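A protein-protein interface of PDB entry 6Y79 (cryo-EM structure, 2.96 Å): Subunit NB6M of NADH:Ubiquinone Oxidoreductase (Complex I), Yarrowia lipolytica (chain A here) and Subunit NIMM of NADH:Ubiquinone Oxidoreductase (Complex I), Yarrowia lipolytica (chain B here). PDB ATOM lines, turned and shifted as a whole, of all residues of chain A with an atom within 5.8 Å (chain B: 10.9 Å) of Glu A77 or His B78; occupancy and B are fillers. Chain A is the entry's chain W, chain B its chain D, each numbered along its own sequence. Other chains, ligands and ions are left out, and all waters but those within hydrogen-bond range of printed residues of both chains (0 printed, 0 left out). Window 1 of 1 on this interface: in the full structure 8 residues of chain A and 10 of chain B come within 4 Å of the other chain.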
ATOM      1  N   LEU A  73      -2.163  32.921   5.238  1.00  0.00           N
ATOM      2  CA  LEU A  73      -2.059  31.862   4.240  1.00  0.00           C
ATOM      3  C   LEU A  73      -2.889  32.172   3.004  1.00  0.00           C
ATOM      4  O   LEU A  73      -2.603  31.660   1.912  1.00  0.00           O
ATOM      5  CB  LEU A  73      -2.502  30.541   4.853  1.00  0.00           C
ATOM      6  CG  LEU A  73      -1.772  30.173   6.137  1.00  0.00           C
ATOM      7  CD1 LEU A  73      -2.459  29.031   6.810  1.00  0.00           C
ATOM      8  CD2 LEU A  73      -0.351  29.810   5.818  1.00  0.00           C
ATOM      9  N   GLN A  74      -3.916  33.007   3.157  1.00  0.00           N
ATOM     10  CA  GLN A  74      -4.744  33.375   2.019  1.00  0.00           C
ATOM     11  C   GLN A  74      -3.995  34.279   1.051  1.00  0.00           C
ATOM     12  O   GLN A  74      -4.125  34.123  -0.168  1.00  0.00           O
ATOM     13  CB  GLN A  74      -6.027  34.044   2.500  1.00  0.00           C
ATOM     14  CG  GLN A  74      -7.055  34.207   1.413  1.00  0.00           C
ATOM     15  CD  GLN A  74      -7.375  32.895   0.739  1.00  0.00           C
ATOM     16  OE1 GLN A  74      -7.639  31.896   1.399  1.00  0.00           O
ATOM     17  NE2 GLN A  74      -7.352  32.888  -0.586  1.00  0.00           N
ATOM     18  N   ALA A  75      -3.199  35.216   1.577  1.00  0.00           N
ATOM     19  CA  ALA A  75      -2.323  36.027   0.738  1.00  0.00           C
ATOM     20  C   ALA A  75      -1.327  35.162  -0.024  1.00  0.00           C
ATOM     21  O   ALA A  75      -1.033  35.436  -1.199  1.00  0.00           O
ATOM     22  CB  ALA A  75      -1.602  37.055   1.603  1.00  0.00           C
ATOM     23  N   GLU A  76      -0.846  34.092   0.621  1.00  0.00           N
ATOM     24  CA  GLU A  76       0.055  33.131  -0.014  1.00  0.00           C
ATOM     25  C   GLU A  76      -0.576  32.466  -1.215  1.00  0.00           C
ATOM     26  O   GLU A  76      -0.009  32.454  -2.321  1.00  0.00           O
ATOM     27  CB  GLU A  76       0.437  32.023   0.958  1.00  0.00           C
ATOM     28  CG  GLU A  76       1.327  31.053   0.329  1.00  0.00           C
ATOM     29  CD  GLU A  76       2.730  31.540   0.298  1.00  0.00           C
ATOM     30  OE1 GLU A  76       3.018  32.340   1.190  1.00  0.00           O
ATOM     31  OE2 GLU A  76       3.488  31.177  -0.619  1.00  0.00           O
ATOM     32  N   GLU A  77      -1.716  31.833  -0.985  1.00  0.00           N
ATOM     33  CA  GLU A  77      -2.342  31.083  -2.062  1.00  0.00           C
ATOM     34  C   GLU A  77      -2.888  32.013  -3.138  1.00  0.00           C
ATOM     35  O   GLU A  77      -2.965  31.624  -4.308  1.00  0.00           O
ATOM     36  CB  GLU A  77      -3.432  30.166  -1.511  1.00  0.00           C
ATOM     37  CG  GLU A  77      -2.859  29.032  -0.682  1.00  0.00           C
ATOM     38  CD  GLU A  77      -2.057  28.025  -1.496  1.00  0.00           C
ATOM     39  OE1 GLU A  77      -0.823  28.184  -1.632  1.00  0.00           O
ATOM     40  OE2 GLU A  77      -2.670  27.062  -1.998  1.00  0.00           O
ATOM     41  N   ASP A  78      -3.172  33.267  -2.781  1.00  0.00           N
ATOM     42  CA  ASP A  78      -3.569  34.252  -3.780  1.00  0.00           C
ATOM     43  C   ASP A  78      -2.413  34.606  -4.709  1.00  0.00           C
ATOM     44  O   ASP A  78      -2.591  34.671  -5.932  1.00  0.00           O
ATOM     45  CB  ASP A  78      -4.111  35.499  -3.092  1.00  0.00           C
ATOM     46  CG  ASP A  78      -5.615  35.463  -2.932  1.00  0.00           C
ATOM     47  OD1 ASP A  78      -6.229  34.415  -3.228  1.00  0.00           O
ATOM     48  OD2 ASP A  78      -6.188  36.487  -2.515  1.00  0.00           O
ATOM     49  N   ARG A  79      -1.217  34.827  -4.147  1.00  0.00           N
ATOM     50  CA  ARG A  79      -0.060  35.107  -4.995  1.00  0.00           C
ATOM     51  C   ARG A  79       0.323  33.906  -5.847  1.00  0.00           C
ATOM     52  O   ARG A  79       0.703  34.079  -7.016  1.00  0.00           O
ATOM     53  CB  ARG A  79       1.123  35.553  -4.146  1.00  0.00           C
ATOM     54  CG  ARG A  79       0.997  36.978  -3.657  1.00  0.00           C
ATOM     55  CD  ARG A  79       2.112  37.330  -2.710  1.00  0.00           C
ATOM     56  NE  ARG A  79       2.000  36.591  -1.460  1.00  0.00           N
ATOM     57  CZ  ARG A  79       3.013  36.376  -0.633  1.00  0.00           C
ATOM     58  NH1 ARG A  79       4.218  36.839  -0.926  1.00  0.00           N
ATOM     59  NH2 ARG A  79       2.826  35.691   0.484  1.00  0.00           N
ATOM     60  N   GLN A  80       0.193  32.692  -5.300  1.00  0.00           N
ATOM     61  CA  GLN A  80       0.448  31.499  -6.106  1.00  0.00           C
ATOM     62  C   GLN A  80      -0.555  31.372  -7.247  1.00  0.00           C
ATOM     63  O   GLN A  80      -0.176  31.034  -8.376  1.00  0.00           O
ATOM     64  CB  GLN A  80       0.416  30.245  -5.234  1.00  0.00           C
ATOM     65  CG  GLN A  80       1.557  30.129  -4.236  1.00  0.00           C
ATOM     66  CD  GLN A  80       2.923  30.152  -4.887  1.00  0.00           C
ATOM     67  OE1 GLN A  80       3.128  29.592  -5.963  1.00  0.00           O
ATOM     68  NE2 GLN A  80       3.872  30.804  -4.233  1.00  0.00           N
ATOM     69  N   THR A  81      -1.826  31.691  -6.981  1.00  0.00           N
ATOM     70  CA  THR A  81      -2.862  31.622  -8.009  1.00  0.00           C
ATOM     71  C   THR A  81      -2.602  32.624  -9.127  1.00  0.00           C
ATOM     72  O   THR A  81      -2.678  32.274 -10.316  1.00  0.00           O
ATOM     73  CB  THR A  81      -4.234  31.862  -7.375  1.00  0.00           C
ATOM     74  OG1 THR A  81      -4.485  30.857  -6.382  1.00  0.00           O
ATOM     75  CG2 THR A  81      -5.329  31.803  -8.416  1.00  0.00           C
ATOM     76  N   VAL A  82      -2.240  33.861  -8.756  1.00  0.00           N
ATOM     77  CA  VAL A  82      -1.966  34.915  -9.733  1.00  0.00           C
ATOM     78  C   VAL A  82      -0.789  34.530 -10.613  1.00  0.00           C
ATOM     79  O   VAL A  82      -0.867  34.604 -11.847  1.00  0.00           O
ATOM     80  CB  VAL A  82      -1.711  36.255  -9.024  1.00  0.00           C
ATOM     81  CG1 VAL A  82      -1.123  37.272  -9.970  1.00  0.00           C
ATOM     82  CG2 VAL A  82      -2.996  36.782  -8.447  1.00  0.00           C
ATOM     83  N   ARG A  83       0.298  34.060  -9.998  1.00  0.00           N
ATOM     84  CA  ARG A  83       1.490  33.703 -10.765  1.00  0.00           C
ATOM     85  C   ARG A  83       1.258  32.529 -11.713  1.00  0.00           C
ATOM     86  O   ARG A  83       1.550  32.640 -12.910  1.00  0.00           O
ATOM     87  CB  ARG A  83       2.634  33.395  -9.815  1.00  0.00           C
ATOM     88  CG  ARG A  83       3.889  33.038 -10.551  1.00  0.00           C
ATOM     89  CD  ARG A  83       4.962  32.608  -9.579  1.00  0.00           C
ATOM     90  NE  ARG A  83       4.596  31.423  -8.799  1.00  0.00           N
ATOM     91  CZ  ARG A  83       4.835  30.159  -9.149  1.00  0.00           C
ATOM     92  NH1 ARG A  83       4.458  29.193  -8.322  1.00  0.00           N
ATOM     93  NH2 ARG A  83       5.449  29.842 -10.289  1.00  0.00           N
ATOM     94  N   ARG A  84       0.640  31.441 -11.228  1.00  0.00           N
ATOM     95  CA  ARG A  84       0.486  30.266 -12.083  1.00  0.00           C
ATOM     96  C   ARG A  84      -0.551  30.482 -13.176  1.00  0.00           C
ATOM     97  O   ARG A  84      -0.412  29.928 -14.273  1.00  0.00           O
ATOM     98  CB  ARG A  84       0.116  29.055 -11.250  1.00  0.00           C
ATOM     99  CG  ARG A  84       1.121  28.730 -10.184  1.00  0.00           C
ATOM    100  CD  ARG A  84       0.619  27.618  -9.348  1.00  0.00           C
ATOM    101  NE  ARG A  84       0.407  26.483 -10.215  1.00  0.00           N
ATOM    102  CZ  ARG A  84       1.218  25.443 -10.260  1.00  0.00           C
ATOM    103  NH1 ARG A  84       0.983  24.446 -11.092  1.00  0.00           N
ATOM    104  NH2 ARG A  84       2.264  25.407  -9.460  1.00  0.00           N
ATOM    105  N   TRP B  45      -8.354  21.214   7.163  1.00  0.00           N
ATOM    106  CA  TRP B  45      -7.406  22.290   7.443  1.00  0.00           C
ATOM    107  C   TRP B  45      -6.042  21.746   7.834  1.00  0.00           C
ATOM    108  O   TRP B  45      -5.014  22.217   7.341  1.00  0.00           O
ATOM    109  CB  TRP B  45      -7.960  23.169   8.560  1.00  0.00           C
ATOM    110  CG  TRP B  45      -7.086  24.299   8.991  1.00  0.00           C
ATOM    111  CD1 TRP B  45      -6.142  24.284   9.971  1.00  0.00           C
ATOM    112  CD2 TRP B  45      -7.116  25.631   8.487  1.00  0.00           C
ATOM    113  NE1 TRP B  45      -5.563  25.520  10.092  1.00  0.00           N
ATOM    114  CE2 TRP B  45      -6.147  26.367   9.190  1.00  0.00           C
ATOM    115  CE3 TRP B  45      -7.855  26.270   7.493  1.00  0.00           C
ATOM    116  CZ2 TRP B  45      -5.905  27.708   8.934  1.00  0.00           C
ATOM    117  CZ3 TRP B  45      -7.622  27.595   7.248  1.00  0.00           C
ATOM    118  CH2 TRP B  45      -6.651  28.303   7.959  1.00  0.00           C
ATOM    119  N   SER B  47      -4.930  18.707   7.192  1.00  0.00           N
ATOM    120  CA  SER B  47      -4.403  18.037   6.004  1.00  0.00           C
ATOM    121  C   SER B  47      -3.672  19.023   5.095  1.00  0.00           C
ATOM    122  O   SER B  47      -2.543  18.757   4.646  1.00  0.00           O
ATOM    123  CB  SER B  47      -5.535  17.359   5.235  1.00  0.00           C
ATOM    124  OG  SER B  47      -6.204  16.383   6.013  1.00  0.00           O
ATOM    125  N   GLN B  48      -4.296  20.181   4.843  1.00  0.00           N
ATOM    126  CA  GLN B  48      -3.659  21.223   4.041  1.00  0.00           C
ATOM    127  C   GLN B  48      -2.445  21.804   4.752  1.00  0.00           C
ATOM    128  O   GLN B  48      -1.472  22.230   4.121  1.00  0.00           O
ATOM    129  CB  GLN B  48      -4.664  22.318   3.721  1.00  0.00           C
ATOM    130  CG  GLN B  48      -5.727  21.914   2.750  1.00  0.00           C
ATOM    131  CD  GLN B  48      -6.692  23.035   2.483  1.00  0.00           C
ATOM    132  OE1 GLN B  48      -6.578  24.112   3.056  1.00  0.00           O
ATOM    133  NE2 GLN B  48      -7.650  22.791   1.609  1.00  0.00           N
ATOM    134  N   MET B  49      -2.469  21.807   6.069  1.00  0.00           N
ATOM    135  CA  MET B  49      -1.334  22.342   6.812  1.00  0.00           C
ATOM    136  C   MET B  49      -0.145  21.385   6.786  1.00  0.00           C
ATOM    137  O   MET B  49       1.013  21.815   6.671  1.00  0.00           O
ATOM    138  CB  MET B  49      -1.754  22.651   8.243  1.00  0.00           C
ATOM    139  CG  MET B  49      -0.779  23.513   8.911  1.00  0.00           C
ATOM    140  SD  MET B  49      -0.518  25.096   8.110  1.00  0.00           S
ATOM    141  CE  MET B  49      -1.959  25.930   8.713  1.00  0.00           C
ATOM    142  N   GLU B  51       0.508  19.221   4.269  1.00  0.00           N
ATOM    143  CA  GLU B  51       1.135  19.298   2.946  1.00  0.00           C
ATOM    144  C   GLU B  51       1.904  20.606   2.767  1.00  0.00           C
ATOM    145  O   GLU B  51       2.943  20.626   2.092  1.00  0.00           O
ATOM    146  CB  GLU B  51       0.104  19.098   1.836  1.00  0.00           C
ATOM    147  CG  GLU B  51      -0.848  20.234   1.715  1.00  0.00           C
ATOM    148  CD  GLU B  51      -2.014  20.025   0.824  1.00  0.00           C
ATOM    149  OE1 GLU B  51      -2.201  18.952   0.184  1.00  0.00           O
ATOM    150  OE2 GLU B  51      -2.888  20.952   0.826  1.00  0.00           O
ATOM    151  N   ARG B  52       1.467  21.686   3.432  1.00  0.00           N
ATOM    152  CA  ARG B  52       2.227  22.932   3.359  1.00  0.00           C
ATOM    153  C   ARG B  52       3.561  22.816   4.088  1.00  0.00           C
ATOM    154  O   ARG B  52       4.587  23.339   3.633  1.00  0.00           O
ATOM    155  CB  ARG B  52       1.408  24.080   3.939  1.00  0.00           C
ATOM    156  CG  ARG B  52       2.085  25.404   3.844  1.00  0.00           C
ATOM    157  CD  ARG B  52       1.266  26.482   4.474  1.00  0.00           C
ATOM    158  NE  ARG B  52       1.962  27.756   4.388  1.00  0.00           N
ATOM    159  CZ  ARG B  52       2.831  28.189   5.289  1.00  0.00           C
ATOM    160  NH1 ARG B  52       3.112  27.455   6.355  1.00  0.00           N
ATOM    161  NH2 ARG B  52       3.416  29.362   5.122  1.00  0.00           N
ATOM    162  N   ASP B  53       3.577  22.098   5.202  1.00  0.00           N
ATOM    163  CA  ASP B  53       4.827  21.966   5.938  1.00  0.00           C
ATOM    164  C   ASP B  53       5.773  20.971   5.282  1.00  0.00           C
ATOM    165  O   ASP B  53       6.994  21.132   5.382  1.00  0.00           O
ATOM    166  CB  ASP B  53       4.547  21.585   7.377  1.00  0.00           C
ATOM    167  CG  ASP B  53       3.701  22.606   8.073  1.00  0.00           C
ATOM    168  OD1 ASP B  53       3.466  23.703   7.515  1.00  0.00           O
ATOM    169  OD2 ASP B  53       3.262  22.296   9.182  1.00  0.00           O
ATOM    170  N   LEU B  54       5.241  19.953   4.590  1.00  0.00           N
ATOM    171  CA  LEU B  54       6.100  19.126   3.743  1.00  0.00           C
ATOM    172  C   LEU B  54       6.690  19.942   2.604  1.00  0.00           C
ATOM    173  O   LEU B  54       7.821  19.687   2.180  1.00  0.00           O
ATOM    174  CB  LEU B  54       5.319  17.928   3.193  1.00  0.00           C
ATOM    175  CG  LEU B  54       5.965  16.778   2.410  1.00  0.00           C
ATOM    176  CD1 LEU B  54       5.125  15.537   2.616  1.00  0.00           C
ATOM    177  CD2 LEU B  54       6.125  17.007   0.915  1.00  0.00           C
ATOM    178  N   ARG B  55       5.940  20.920   2.099  1.00  0.00           N
ATOM    179  CA  ARG B  55       6.486  21.811   1.084  1.00  0.00           C
ATOM    180  C   ARG B  55       7.567  22.722   1.644  1.00  0.00           C
ATOM    181  O   ARG B  55       8.542  23.023   0.950  1.00  0.00           O
ATOM    182  CB  ARG B  55       5.356  22.645   0.478  1.00  0.00           C
ATOM    183  CG  ARG B  55       5.723  23.443  -0.739  1.00  0.00           C
ATOM    184  CD  ARG B  55       4.485  23.793  -1.523  1.00  0.00           C
ATOM    185  NE  ARG B  55       3.437  24.337  -0.672  1.00  0.00           N
ATOM    186  CZ  ARG B  55       3.191  25.634  -0.532  1.00  0.00           C
ATOM    187  NH1 ARG B  55       3.927  26.521  -1.183  1.00  0.00           N
ATOM    188  NH2 ARG B  55       2.213  26.043   0.261  1.00  0.00           N
ATOM    189  N   LEU B  56       7.421  23.149   2.894  1.00  0.00           N
ATOM    190  CA  LEU B  56       8.309  24.174   3.426  1.00  0.00           C
ATOM    191  C   LEU B  56       9.589  23.580   4.007  1.00  0.00           C
ATOM    192  O   LEU B  56      10.658  24.182   3.888  1.00  0.00           O
ATOM    193  CB  LEU B  56       7.570  24.998   4.471  1.00  0.00           C
ATOM    194  CG  LEU B  56       8.270  26.145   5.181  1.00  0.00           C
ATOM    195  CD1 LEU B  56       8.975  27.082   4.221  1.00  0.00           C
ATOM    196  CD2 LEU B  56       7.184  26.870   5.915  1.00  0.00           C
ATOM    197  N   PRO B  71      12.675  29.972   2.193  1.00  0.00           N
ATOM    198  CA  PRO B  71      13.715  29.884   1.155  1.00  0.00           C
ATOM    199  C   PRO B  71      13.312  30.308  -0.251  1.00  0.00           C
ATOM    200  O   PRO B  71      12.199  30.783  -0.501  1.00  0.00           O
ATOM    201  CB  PRO B  71      14.083  28.396   1.169  1.00  0.00           C
ATOM    202  CG  PRO B  71      13.766  27.950   2.520  1.00  0.00           C
ATOM    203  CD  PRO B  71      12.542  28.690   2.913  1.00  0.00           C
ATOM    204  N   GLU B  72      14.254  30.117  -1.179  1.00  0.00           N
ATOM    205  CA  GLU B  72      14.126  30.516  -2.576  1.00  0.00           C
ATOM    206  C   GLU B  72      13.266  29.559  -3.383  1.00  0.00           C
ATOM    207  O   GLU B  72      12.420  30.010  -4.163  1.00  0.00           O
ATOM    208  CB  GLU B  72      15.520  30.618  -3.216  1.00  0.00           C
ATOM    209  CG  GLU B  72      15.596  31.266  -4.614  1.00  0.00           C
ATOM    210  CD  GLU B  72      15.366  30.286  -5.767  1.00  0.00           C
ATOM    211  OE1 GLU B  72      15.647  29.081  -5.599  1.00  0.00           O
ATOM    212  OE2 GLU B  72      14.908  30.727  -6.840  1.00  0.00           O
ATOM    213  N   ALA B  73      13.455  28.249  -3.213  1.00  0.00           N
ATOM    214  CA  ALA B  73      12.665  27.279  -3.961  1.00  0.00           C
ATOM    215  C   ALA B  73      11.260  27.113  -3.403  1.00  0.00           C
ATOM    216  O   ALA B  73      10.457  26.385  -3.994  1.00  0.00           O
ATOM    217  CB  ALA B  73      13.377  25.927  -3.985  1.00  0.00           C
ATOM    218  N   PHE B  74      10.951  27.771  -2.286  1.00  0.00           N
ATOM    219  CA  PHE B  74       9.631  27.661  -1.684  1.00  0.00           C
ATOM    220  C   PHE B  74       8.574  28.392  -2.498  1.00  0.00           C
ATOM    221  O   PHE B  74       7.411  27.978  -2.511  1.00  0.00           O
ATOM    222  CB  PHE B  74       9.665  28.201  -0.259  1.00  0.00           C
ATOM    223  CG  PHE B  74       8.344  28.155   0.427  1.00  0.00           C
ATOM    224  CD1 PHE B  74       7.793  26.946   0.804  1.00  0.00           C
ATOM    225  CD2 PHE B  74       7.638  29.314   0.672  1.00  0.00           C
ATOM    226  CE1 PHE B  74       6.570  26.897   1.435  1.00  0.00           C
ATOM    227  CE2 PHE B  74       6.412  29.269   1.302  1.00  0.00           C
ATOM    228  CZ  PHE B  74       5.880  28.060   1.682  1.00  0.00           C
ATOM    229  N   LYS B  75       8.943  29.474  -3.180  1.00  0.00           N
ATOM    230  CA  LYS B  75       7.968  30.160  -4.017  1.00  0.00           C
ATOM    231  C   LYS B  75       7.686  29.401  -5.306  1.00  0.00           C
ATOM    232  O   LYS B  75       6.694  29.695  -5.977  1.00  0.00           O
ATOM    233  CB  LYS B  75       8.441  31.573  -4.356  1.00  0.00           C
ATOM    234  CG  LYS B  75       8.653  32.503  -3.176  1.00  0.00           C
ATOM    235  CD  LYS B  75       8.965  33.911  -3.672  1.00  0.00           C
ATOM    236  CE  LYS B  75       9.410  34.835  -2.556  1.00  0.00           C
ATOM    237  NZ  LYS B  75       9.778  36.212  -2.957  1.00  0.00           N
ATOM    238  N   HIS B  76       8.522  28.424  -5.659  1.00  0.00           N
ATOM    239  CA  HIS B  76       8.414  27.722  -6.929  1.00  0.00           C
ATOM    240  C   HIS B  76       8.011  26.260  -6.809  1.00  0.00           C
ATOM    241  O   HIS B  76       7.699  25.646  -7.834  1.00  0.00           O
ATOM    242  CB  HIS B  76       9.743  27.795  -7.691  1.00  0.00           C
ATOM    243  CG  HIS B  76      10.121  29.179  -8.119  1.00  0.00           C
ATOM    244  ND1 HIS B  76      10.884  30.020  -7.340  1.00  0.00           N
ATOM    245  CD2 HIS B  76       9.844  29.863  -9.252  1.00  0.00           C
ATOM    246  CE1 HIS B  76      11.058  31.166  -7.974  1.00  0.00           C
ATOM    247  NE2 HIS B  76      10.435  31.097  -9.137  1.00  0.00           N
ATOM    248  N   ASN B  77       8.019  25.672  -5.614  1.00  0.00           N
ATOM    249  CA  ASN B  77       7.647  24.271  -5.481  1.00  0.00           C
ATOM    250  C   ASN B  77       6.171  24.083  -5.151  1.00  0.00           C
ATOM    251  O   ASN B  77       5.788  23.022  -4.652  1.00  0.00           O
ATOM    252  CB  ASN B  77       8.530  23.562  -4.443  1.00  0.00           C
ATOM    253  CG  ASN B  77       8.432  24.159  -3.045  1.00  0.00           C
ATOM    254  OD1 ASN B  77       7.765  25.162  -2.815  1.00  0.00           O
ATOM    255  ND2 ASN B  77       9.114  23.529  -2.099  1.00  0.00           N
ATOM    256  N   HIS B  78       5.341  25.085  -5.427  1.00  0.00           N
ATOM    257  CA  HIS B  78       3.935  25.030  -5.060  1.00  0.00           C
ATOM    258  C   HIS B  78       3.150  24.133  -6.005  1.00  0.00           C
ATOM    259  O   HIS B  78       3.405  24.103  -7.201  1.00  0.00           O
ATOM    260  CB  HIS B  78       3.326  26.428  -5.058  1.00  0.00           C
ATOM    261  CG  HIS B  78       1.856  26.422  -4.811  1.00  0.00           C
ATOM    262  ND1 HIS B  78       1.308  25.908  -3.658  1.00  0.00           N
ATOM    263  CD2 HIS B  78       0.817  26.791  -5.592  1.00  0.00           C
ATOM    264  CE1 HIS B  78      -0.007  25.999  -3.723  1.00  0.00           C
ATOM    265  NE2 HIS B  78      -0.331  26.534  -4.885  1.00  0.00           N
ATOM    266  N   VAL B  79       2.161  23.435  -5.465  1.00  0.00           N
ATOM    267  CA  VAL B  79       1.454  22.364  -6.148  1.00  0.00           C
ATOM    268  C   VAL B  79      -0.011  22.742  -6.350  1.00  0.00           C
ATOM    269  O   VAL B  79      -0.645  23.311  -5.456  1.00  0.00           O
ATOM    270  CB  VAL B  79       1.617  21.072  -5.321  1.00  0.00           C
ATOM    271  CG1 VAL B  79       0.530  20.072  -5.594  1.00  0.00           C
ATOM    272  CG2 VAL B  79       2.974  20.473  -5.579  1.00  0.00           C
ATOM    273  N   TRP B  80      -0.529  22.471  -7.545  1.00  0.00           N
ATOM    274  CA  TRP B  80      -1.946  22.258  -7.779  1.00  0.00           C
ATOM    275  C   TRP B  80      -2.167  20.781  -8.061  1.00  0.00           C
ATOM    276  O   TRP B  80      -1.245  20.053  -8.430  1.00  0.00           O
ATOM    277  CB  TRP B  80      -2.458  23.063  -8.970  1.00  0.00           C
ATOM    278  CG  TRP B  80      -2.613  24.506  -8.775  1.00  0.00           C
ATOM    279  CD1 TRP B  80      -2.552  25.191  -7.608  1.00  0.00           C
ATOM    280  CD2 TRP B  80      -2.858  25.467  -9.799  1.00  0.00           C
ATOM    281  NE1 TRP B  80      -2.749  26.529  -7.838  1.00  0.00           N
ATOM    282  CE2 TRP B  80      -2.939  26.723  -9.180  1.00  0.00           C
ATOM    283  CE3 TRP B  80      -3.016  25.385 -11.184  1.00  0.00           C
ATOM    284  CZ2 TRP B  80      -3.171  27.889  -9.897  1.00  0.00           C
ATOM    285  CZ3 TRP B  80      -3.253  26.538 -11.892  1.00  0.00           C
ATOM    286  CH2 TRP B  80      -3.326  27.776 -11.249  1.00  0.00           C
ATOM    287  N   LYS B  81      -3.404  20.338  -7.901  1.00  0.00           N
ATOM    288  CA  LYS B  81      -3.767  18.951  -8.142  1.00  0.00           C
ATOM    289  C   LYS B  81      -4.714  18.900  -9.331  1.00  0.00           C
ATOM    290  O   LYS B  81      -5.765  19.545  -9.313  1.00  0.00           O
ATOM    291  CB  LYS B  81      -4.406  18.340  -6.899  1.00  0.00           C
ATOM    292  CG  LYS B  81      -3.651  18.668  -5.628  1.00  0.00           C
ATOM    293  CD  LYS B  81      -4.256  17.990  -4.426  1.00  0.00           C
ATOM    294  CE  LYS B  81      -3.273  17.969  -3.277  1.00  0.00           C
ATOM    295  NZ  LYS B  81      -3.871  17.427  -2.032  1.00  0.00           N
ATOM    296  N   SER B  82      -4.329  18.163 -10.367  1.00  0.00           N
ATOM    297  CA  SER B  82      -5.149  17.983 -11.557  1.00  0.00           C
ATOM    298  C   SER B  82      -5.802  16.610 -11.489  1.00  0.00           C
ATOM    299  O   SER B  82      -5.132  15.585 -11.630  1.00  0.00           O
ATOM    300  CB  SER B  82      -4.319  18.124 -12.827  1.00  0.00           C
ATOM    301  OG  SER B  82      -3.402  17.057 -12.945  1.00  0.00           O
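NH1 of Arg A83 lies within hydrogen-bond range of O of Lys B75, 3.3 Å away.
The backbone carbonyl oxygen (O) of His B78 sits at hydrogen-bond distance from the guanidinium group (NH2) of Arg A84, at 2.8 Å.
NE2 of Gln A80 is in hydrogen-bond range of O of Lys B75.
The side-chain amide oxygen of Gln A80 lies within hydrogen-bond range of the guanidinium group of Arg A83 (2.7 Å).
The side-chain hydroxyl (OG1) of Thr A81 is in hydrogen-bond range of the backbone carbonyl oxygen (O) of Glu A77.
The side-chain amide oxygen of Asn B77 sits close to the backbone carbonyl oxygen of Phe B74.
OE1 of Glu A76 is in salt-bridge range of NH2 of Arg A79 (3.4 Å).
The guanidinium group of Arg B52 lies within salt-bridge range of the side-chain carboxylate of Asp B53 (3.9 Å).
Among the printed residues, pairs that only touch across the chains: Glu A77 with His B78 (3.1 Å), Gln A80 with His B78 (3.3 Å), Leu A73 with Arg B52 (3.4 Å), Arg A84 with Trp B80 (3.4 Å), Leu A73 with Met B49 (3.7 Å) and Glu A76 with Phe B74 (3.99 Å).
Glu A77 touches just one residue of chain B: His B78 (3.1 Å).
His B78 touches three residues of chain A.
No residue of chain B comes within 4 Å of Gln A74.
Of chain B, only Lys B75 and His B78 come within 4 Å of Gln A80.
Of the printed residues of chain B, Leu A73 touches Met B49 and Arg B52.
Printed residues of chain A within 4 Å of Trp B80: Arg A84 (3.4 Å).
Lys B81 touches none of the printed residues of chain A.
The nearest residue of chain B that does not touch Glu A77 is Arg B55 (4.2 Å).
The nearest printed residue of chain A that does not touch Phe B74 is Gln A80 (4.8 Å).
Of the 12 printed residues of chain A, 6 touch a printed residue of chain B.
Hydrophobic or aromatic side chains of chain A within 4 Å of the printed part of chain B: Leu A73.
Among the printed residues, 9 pairs touch across the chains.
Among the printed residues, no Asp or Glu carboxylate lies within 4 Å of a Lys or Arg side-chain nitrogen of the other chain.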
